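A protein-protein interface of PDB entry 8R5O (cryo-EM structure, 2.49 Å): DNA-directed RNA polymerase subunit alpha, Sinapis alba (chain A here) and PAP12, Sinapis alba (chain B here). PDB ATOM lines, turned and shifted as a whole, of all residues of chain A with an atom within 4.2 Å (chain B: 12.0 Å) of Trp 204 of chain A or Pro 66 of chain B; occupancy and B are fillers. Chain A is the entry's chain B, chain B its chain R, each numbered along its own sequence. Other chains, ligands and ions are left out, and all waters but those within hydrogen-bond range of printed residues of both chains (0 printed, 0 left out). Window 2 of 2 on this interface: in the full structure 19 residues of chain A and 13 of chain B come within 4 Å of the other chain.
Printed residues of chain A that touch a printed residue of chain B: Tyr 29, Gln 180, Asn 181, Glu 202 and Trp 204. Hydrophobic or aromatic side chains of chain A that line the printed part of chain B: Tyr 29 and Trp 204. Of the 9 printed residues of chain B, 5 touch a printed residue of chain A. Printed residues of chain B that touch a printed residue of chain A: Pro 66, Phe 67, Glu 69, Glu 70 and Arg 73. Hydrophobic or aromatic side chains of chain B that line the printed part of chain A: Phe 67. Among the printed residues, 9 pairs touch across the chains.
Glu 69 of chain B touches Tyr 29 of chain A (OE2 to CG, 3.8 Å). Phe 67 of chain B touches Gln 180 of chain A. Phe 67 of chain B touches Asn 181 of chain A (CD1 to CB, 3.997 Å). Glu 70 of chain B touches Glu 202 of chain A. Trp 204 of chain A touches Pro 66 of chain B (NE1 to O, 3.7 Å). Phe 67 of chain B touches Trp 204 of chain A (CD1 to CD1, 3.3 Å).
OE2 of Glu 202 of chain A is in hydrogen-bond range of OH of Tyr 29 of chain A (2.7 Å). The backbone NH of Gln 180 of chain A lies within hydrogen-bond range of the backbone carbonyl oxygen of Trp 204 of chain A (2.6 Å). The backbone carbonyl oxygen (O) of Asn 181 of chain A is in hydrogen-bond range of the backbone NH (N) of Trp 204 of chain A, 2.9 Å away. The side-chain carboxylate (OE2) of Glu 70 of chain B is in salt-bridge range of the guanidinium group (NH1) of Arg 73 of chain B (3.2 Å). The side-chain carboxylate of Glu 70 of chain B is in salt-bridge range of the side-chain amino group of Lys 74 of chain B (3.98 Å).
NH2 of Arg 73 of chain B is in hydrogen-bond range of OH of Tyr 29 of chain A, 3.0 Å away. OE2 of Glu 202 of chain A lies within salt-bridge range of NH2 of Arg 73 of chain B, 2.4 Å away. The side-chain carboxylate (OE1) of Glu 69 of chain B is in hydrogen-bond range of the indole nitrogen (NE1) of Trp 204 of chain A (2.9 Å).
Tyr 29 of chain A touches just these residues of chain B: Glu 69 and Arg 73. No residue of chain B comes within 4 Å of Val 179 of chain A. Gln 180 of chain A touches just one residue of chain B: Phe 67. Of the printed residues of chain B, Asn 181 of chain A touches Phe 67. Ala 182 of chain A touches none of the printed residues of chain B. Glu 202 of chain A touches just these residues of chain B: Glu 70 (3.1 Å) and Arg 73 (2.4 Å). Trp 204 of chain A touches three residues of chain B. Thr 205 of chain A touches none of the printed residues of chain B. Of the printed residues of chain A, Pro 66 of chain B touches Trp 204. Printed residues of chain A within 4 Å of Glu 69 of chain B: Tyr 29 and Trp 204. Val 72 of chain B touches none of the printed residues of chain A. Of the printed residues of chain A, Arg 73 of chain B touches Tyr 29 (3.0 Å) and Glu 202 (2.4 Å). The nearest printed residue of chain A that does not touch Pro 66 of chain B is Tyr 29 of chain A (6.2 Å).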
ATOM      1  N   TYR A  28      28.871  13.725  27.152  1.00  0.00           N
ATOM      2  CA  TYR A  28      27.795  13.892  26.186  1.00  0.00           C
ATOM      3  C   TYR A  28      27.922  12.829  25.104  1.00  0.00           C
ATOM      4  O   TYR A  28      29.020  12.567  24.605  1.00  0.00           O
ATOM      5  CB  TYR A  28      27.816  15.283  25.542  1.00  0.00           C
ATOM      6  CG  TYR A  28      27.469  16.438  26.461  1.00  0.00           C
ATOM      7  CD1 TYR A  28      27.376  16.265  27.836  1.00  0.00           C
ATOM      8  CD2 TYR A  28      27.221  17.702  25.948  1.00  0.00           C
ATOM      9  CE1 TYR A  28      27.058  17.315  28.669  1.00  0.00           C
ATOM     10  CE2 TYR A  28      26.900  18.761  26.778  1.00  0.00           C
ATOM     11  CZ  TYR A  28      26.819  18.560  28.137  1.00  0.00           C
ATOM     12  OH  TYR A  28      26.502  19.607  28.972  1.00  0.00           O
ATOM     13  N   TYR A  29      26.798  12.223  24.740  1.00  0.00           N
ATOM     14  CA  TYR A  29      26.768  11.201  23.707  1.00  0.00           C
ATOM     15  C   TYR A  29      25.764  11.585  22.632  1.00  0.00           C
ATOM     16  O   TYR A  29      24.699  12.130  22.932  1.00  0.00           O
ATOM     17  CB  TYR A  29      26.415   9.825  24.289  1.00  0.00           C
ATOM     18  CG  TYR A  29      26.147   8.773  23.238  1.00  0.00           C
ATOM     19  CD1 TYR A  29      27.192   8.130  22.591  1.00  0.00           C
ATOM     20  CD2 TYR A  29      24.849   8.422  22.895  1.00  0.00           C
ATOM     21  CE1 TYR A  29      26.952   7.172  21.630  1.00  0.00           C
ATOM     22  CE2 TYR A  29      24.601   7.465  21.933  1.00  0.00           C
ATOM     23  CZ  TYR A  29      25.656   6.842  21.305  1.00  0.00           C
ATOM     24  OH  TYR A  29      25.417   5.886  20.347  1.00  0.00           O
ATOM     25  N   VAL A 179      36.542  15.914  21.868  1.00  0.00           N
ATOM     26  CA  VAL A 179      35.835  14.700  21.481  1.00  0.00           C
ATOM     27  C   VAL A 179      36.550  13.518  22.119  1.00  0.00           C
ATOM     28  O   VAL A 179      37.695  13.211  21.772  1.00  0.00           O
ATOM     29  CB  VAL A 179      35.771  14.553  19.954  1.00  0.00           C
ATOM     30  CG1 VAL A 179      35.103  13.243  19.575  1.00  0.00           C
ATOM     31  CG2 VAL A 179      35.036  15.729  19.339  1.00  0.00           C
ATOM     32  N   GLN A 180      35.878  12.856  23.061  1.00  0.00           N
ATOM     33  CA  GLN A 180      36.492  11.748  23.781  1.00  0.00           C
ATOM     34  C   GLN A 180      36.641  10.516  22.900  1.00  0.00           C
ATOM     35  O   GLN A 180      37.647   9.805  22.986  1.00  0.00           O
ATOM     36  CB  GLN A 180      35.667  11.410  25.022  1.00  0.00           C
ATOM     37  CG  GLN A 180      35.452  12.578  25.966  1.00  0.00           C
ATOM     38  CD  GLN A 180      36.725  13.002  26.667  1.00  0.00           C
ATOM     39  OE1 GLN A 180      37.467  13.850  26.174  1.00  0.00           O
ATOM     40  NE2 GLN A 180      36.983  12.412  27.826  1.00  0.00           N
ATOM     41  N   ASN A 181      35.653  10.250  22.051  1.00  0.00           N
ATOM     42  CA  ASN A 181      35.647   9.044  21.241  1.00  0.00           C
ATOM     43  C   ASN A 181      34.705   9.258  20.066  1.00  0.00           C
ATOM     44  O   ASN A 181      33.774  10.062  20.141  1.00  0.00           O
ATOM     45  CB  ASN A 181      35.218   7.826  22.069  1.00  0.00           C
ATOM     46  CG  ASN A 181      35.484   6.514  21.363  1.00  0.00           C
ATOM     47  OD1 ASN A 181      36.459   6.378  20.626  1.00  0.00           O
ATOM     48  ND2 ASN A 181      34.612   5.539  21.584  1.00  0.00           N
ATOM     49  N   ALA A 182      34.962   8.535  18.980  1.00  0.00           N
ATOM     50  CA  ALA A 182      34.135   8.627  17.787  1.00  0.00           C
ATOM     51  C   ALA A 182      34.222   7.317  17.020  1.00  0.00           C
ATOM     52  O   ALA A 182      35.295   6.717  16.925  1.00  0.00           O
ATOM     53  CB  ALA A 182      34.563   9.796  16.895  1.00  0.00           C
ATOM     54  N   GLU A 202      28.862   7.913  15.723  1.00  0.00           N
ATOM     55  CA  GLU A 202      28.739   8.089  17.164  1.00  0.00           C
ATOM     56  C   GLU A 202      29.826   9.030  17.660  1.00  0.00           C
ATOM     57  O   GLU A 202      30.989   8.908  17.268  1.00  0.00           O
ATOM     58  CB  GLU A 202      28.848   6.750  17.895  1.00  0.00           C
ATOM     59  CG  GLU A 202      27.589   5.916  17.866  1.00  0.00           C
ATOM     60  CD  GLU A 202      27.825   4.506  18.361  1.00  0.00           C
ATOM     61  OE1 GLU A 202      28.598   3.776  17.709  1.00  0.00           O
ATOM     62  OE2 GLU A 202      27.252   4.133  19.404  1.00  0.00           O
ATOM     63  N   ILE A 203      29.443   9.971  18.519  1.00  0.00           N
ATOM     64  CA  ILE A 203      30.351  10.992  19.025  1.00  0.00           C
ATOM     65  C   ILE A 203      30.205  11.081  20.539  1.00  0.00           C
ATOM     66  O   ILE A 203      29.085  11.166  21.056  1.00  0.00           O
ATOM     67  CB  ILE A 203      30.082  12.362  18.370  1.00  0.00           C
ATOM     68  CG1 ILE A 203      30.258  12.275  16.854  1.00  0.00           C
ATOM     69  CG2 ILE A 203      30.993  13.424  18.951  1.00  0.00           C
ATOM     70  CD1 ILE A 203      29.915  13.548  16.116  1.00  0.00           C
ATOM     71  N   TRP A 204      31.334  11.050  21.244  1.00  0.00           N
ATOM     72  CA  TRP A 204      31.397  11.294  22.680  1.00  0.00           C
ATOM     73  C   TRP A 204      32.222  12.549  22.924  1.00  0.00           C
ATOM     74  O   TRP A 204      33.361  12.643  22.457  1.00  0.00           O
ATOM     75  CB  TRP A 204      32.029  10.115  23.429  1.00  0.00           C
ATOM     76  CG  TRP A 204      31.230   8.845  23.457  1.00  0.00           C
ATOM     77  CD1 TRP A 204      30.415   8.413  24.461  1.00  0.00           C
ATOM     78  CD2 TRP A 204      31.198   7.825  22.451  1.00  0.00           C
ATOM     79  NE1 TRP A 204      29.869   7.195  24.139  1.00  0.00           N
ATOM     80  CE2 TRP A 204      30.334   6.813  22.910  1.00  0.00           C
ATOM     81  CE3 TRP A 204      31.810   7.673  21.204  1.00  0.00           C
ATOM     82  CZ2 TRP A 204      30.065   5.665  22.167  1.00  0.00           C
ATOM     83  CZ3 TRP A 204      31.544   6.534  20.467  1.00  0.00           C
ATOM     84  CH2 TRP A 204      30.678   5.546  20.949  1.00  0.00           C
ATOM     85  N   THR A 205      31.657  13.507  23.651  1.00  0.00           N
ATOM     86  CA  THR A 205      32.360  14.735  23.991  1.00  0.00           C
ATOM     87  C   THR A 205      32.432  14.895  25.504  1.00  0.00           C
ATOM     88  O   THR A 205      31.667  14.285  26.253  1.00  0.00           O
ATOM     89  CB  THR A 205      31.690  15.972  23.374  1.00  0.00           C
ATOM     90  OG1 THR A 205      30.482  16.269  24.080  1.00  0.00           O
ATOM     91  CG2 THR A 205      31.368  15.741  21.907  1.00  0.00           C
ATOM     92  N   PRO B  66      31.845   4.033  30.141  1.00  0.00           N
ATOM     93  CA  PRO B  66      30.949   5.075  29.631  1.00  0.00           C
ATOM     94  C   PRO B  66      30.880   5.097  28.108  1.00  0.00           C
ATOM     95  O   PRO B  66      30.086   5.849  27.540  1.00  0.00           O
ATOM     96  CB  PRO B  66      31.570   6.371  30.167  1.00  0.00           C
ATOM     97  CG  PRO B  66      32.979   6.018  30.518  1.00  0.00           C
ATOM     98  CD  PRO B  66      32.927   4.594  30.966  1.00  0.00           C
ATOM     99  N   PHE B  67      31.696   4.277  27.459  1.00  0.00           N
ATOM    100  CA  PHE B  67      31.745   4.189  26.005  1.00  0.00           C
ATOM    101  C   PHE B  67      31.330   2.802  25.531  1.00  0.00           C
ATOM    102  O   PHE B  67      31.961   2.211  24.654  1.00  0.00           O
ATOM    103  CB  PHE B  67      33.137   4.539  25.484  1.00  0.00           C
ATOM    104  CG  PHE B  67      33.676   5.829  26.024  1.00  0.00           C
ATOM    105  CD1 PHE B  67      33.287   7.039  25.479  1.00  0.00           C
ATOM    106  CD2 PHE B  67      34.578   5.831  27.074  1.00  0.00           C
ATOM    107  CE1 PHE B  67      33.783   8.228  25.972  1.00  0.00           C
ATOM    108  CE2 PHE B  67      35.077   7.018  27.572  1.00  0.00           C
ATOM    109  CZ  PHE B  67      34.679   8.218  27.018  1.00  0.00           C
ATOM    110  N   VAL B  68      30.264   2.262  26.117  1.00  0.00           N
ATOM    111  CA  VAL B  68      29.788   0.924  25.794  1.00  0.00           C
ATOM    112  C   VAL B  68      28.457   0.955  25.056  1.00  0.00           C
ATOM    113  O   VAL B  68      27.789  -0.079  24.954  1.00  0.00           O
ATOM    114  CB  VAL B  68      29.692   0.045  27.053  1.00  0.00           C
ATOM    115  CG1 VAL B  68      31.071  -0.173  27.657  1.00  0.00           C
ATOM    116  CG2 VAL B  68      28.752   0.672  28.069  1.00  0.00           C
ATOM    117  N   GLU B  69      28.049   2.116  24.538  1.00  0.00           N
ATOM    118  CA  GLU B  69      26.768   2.206  23.840  1.00  0.00           C
ATOM    119  C   GLU B  69      26.743   1.312  22.608  1.00  0.00           C
ATOM    120  O   GLU B  69      25.759   0.606  22.360  1.00  0.00           O
ATOM    121  CB  GLU B  69      26.477   3.654  23.448  1.00  0.00           C
ATOM    122  CG  GLU B  69      25.927   4.505  24.568  1.00  0.00           C
ATOM    123  CD  GLU B  69      26.992   5.319  25.268  1.00  0.00           C
ATOM    124  OE1 GLU B  69      28.190   5.064  25.031  1.00  0.00           O
ATOM    125  OE2 GLU B  69      26.630   6.220  26.053  1.00  0.00           O
ATOM    126  N   GLU B  70      27.816   1.335  21.817  1.00  0.00           N
ATOM    127  CA  GLU B  70      27.868   0.498  20.625  1.00  0.00           C
ATOM    128  C   GLU B  70      27.844  -0.978  20.995  1.00  0.00           C
ATOM    129  O   GLU B  70      27.185  -1.786  20.329  1.00  0.00           O
ATOM    130  CB  GLU B  70      29.117   0.827  19.808  1.00  0.00           C
ATOM    131  CG  GLU B  70      28.929   0.702  18.306  1.00  0.00           C
ATOM    132  CD  GLU B  70      28.696  -0.723  17.854  1.00  0.00           C
ATOM    133  OE1 GLU B  70      29.460  -1.616  18.278  1.00  0.00           O
ATOM    134  OE2 GLU B  70      27.743  -0.950  17.081  1.00  0.00           O
ATOM    135  N   GLN B  71      28.562  -1.349  22.054  1.00  0.00           N
ATOM    136  CA  GLN B  71      28.590  -2.740  22.487  1.00  0.00           C
ATOM    137  C   GLN B  71      27.230  -3.181  23.016  1.00  0.00           C
ATOM    138  O   GLN B  71      26.756  -4.277  22.696  1.00  0.00           O
ATOM    139  CB  GLN B  71      29.674  -2.928  23.548  1.00  0.00           C
ATOM    140  CG  GLN B  71      29.856  -4.357  23.984  1.00  0.00           C
ATOM    141  CD  GLN B  71      30.790  -4.489  25.164  1.00  0.00           C
ATOM    142  OE1 GLN B  71      30.688  -5.437  25.936  1.00  0.00           O
ATOM    143  NE2 GLN B  71      31.707  -3.541  25.307  1.00  0.00           N
ATOM    144  N   VAL B  72      26.584  -2.335  23.822  1.00  0.00           N
ATOM    145  CA  VAL B  72      25.283  -2.685  24.393  1.00  0.00           C
ATOM    146  C   VAL B  72      24.257  -2.899  23.287  1.00  0.00           C
ATOM    147  O   VAL B  72      23.491  -3.869  23.304  1.00  0.00           O
ATOM    148  CB  VAL B  72      24.824  -1.605  25.389  1.00  0.00           C
ATOM    149  CG1 VAL B  72      23.330  -1.714  25.649  1.00  0.00           C
ATOM    150  CG2 VAL B  72      25.594  -1.723  26.691  1.00  0.00           C
ATOM    151  N   ARG B  73      24.234  -1.998  22.304  1.00  0.00           N
ATOM    152  CA  ARG B  73      23.276  -2.123  21.213  1.00  0.00           C
ATOM    153  C   ARG B  73      23.556  -3.351  20.355  1.00  0.00           C
ATOM    154  O   ARG B  73      22.619  -3.964  19.834  1.00  0.00           O
ATOM    155  CB  ARG B  73      23.273  -0.843  20.373  1.00  0.00           C
ATOM    156  CG  ARG B  73      23.462  -1.042  18.880  1.00  0.00           C
ATOM    157  CD  ARG B  73      23.105   0.219  18.108  1.00  0.00           C
ATOM    158  NE  ARG B  73      23.575   1.427  18.775  1.00  0.00           N
ATOM    159  CZ  ARG B  73      24.777   1.960  18.606  1.00  0.00           C
ATOM    160  NH1 ARG B  73      25.672   1.408  17.804  1.00  0.00           N
ATOM    161  NH2 ARG B  73      25.089   3.074  19.260  1.00  0.00           N
ATOM    162  N   LYS B  74      24.825  -3.740  20.215  1.00  0.00           N
ATOM    163  CA  LYS B  74      25.141  -4.945  19.454  1.00  0.00           C
ATOM    164  C   LYS B  74      24.760  -6.205  20.221  1.00  0.00           C
ATOM    165  O   LYS B  74      24.375  -7.211  19.616  1.00  0.00           O
ATOM    166  CB  LYS B  74      26.623  -4.972  19.085  1.00  0.00           C
ATOM    167  CG  LYS B  74      26.978  -4.113  17.886  1.00  0.00           C
ATOM    168  CD  LYS B  74      28.333  -4.496  17.317  1.00  0.00           C
ATOM    169  CE  LYS B  74      28.582  -3.816  15.981  1.00  0.00           C
ATOM    170  NZ  LYS B  74      29.843  -4.283  15.345  1.00  0.00           N
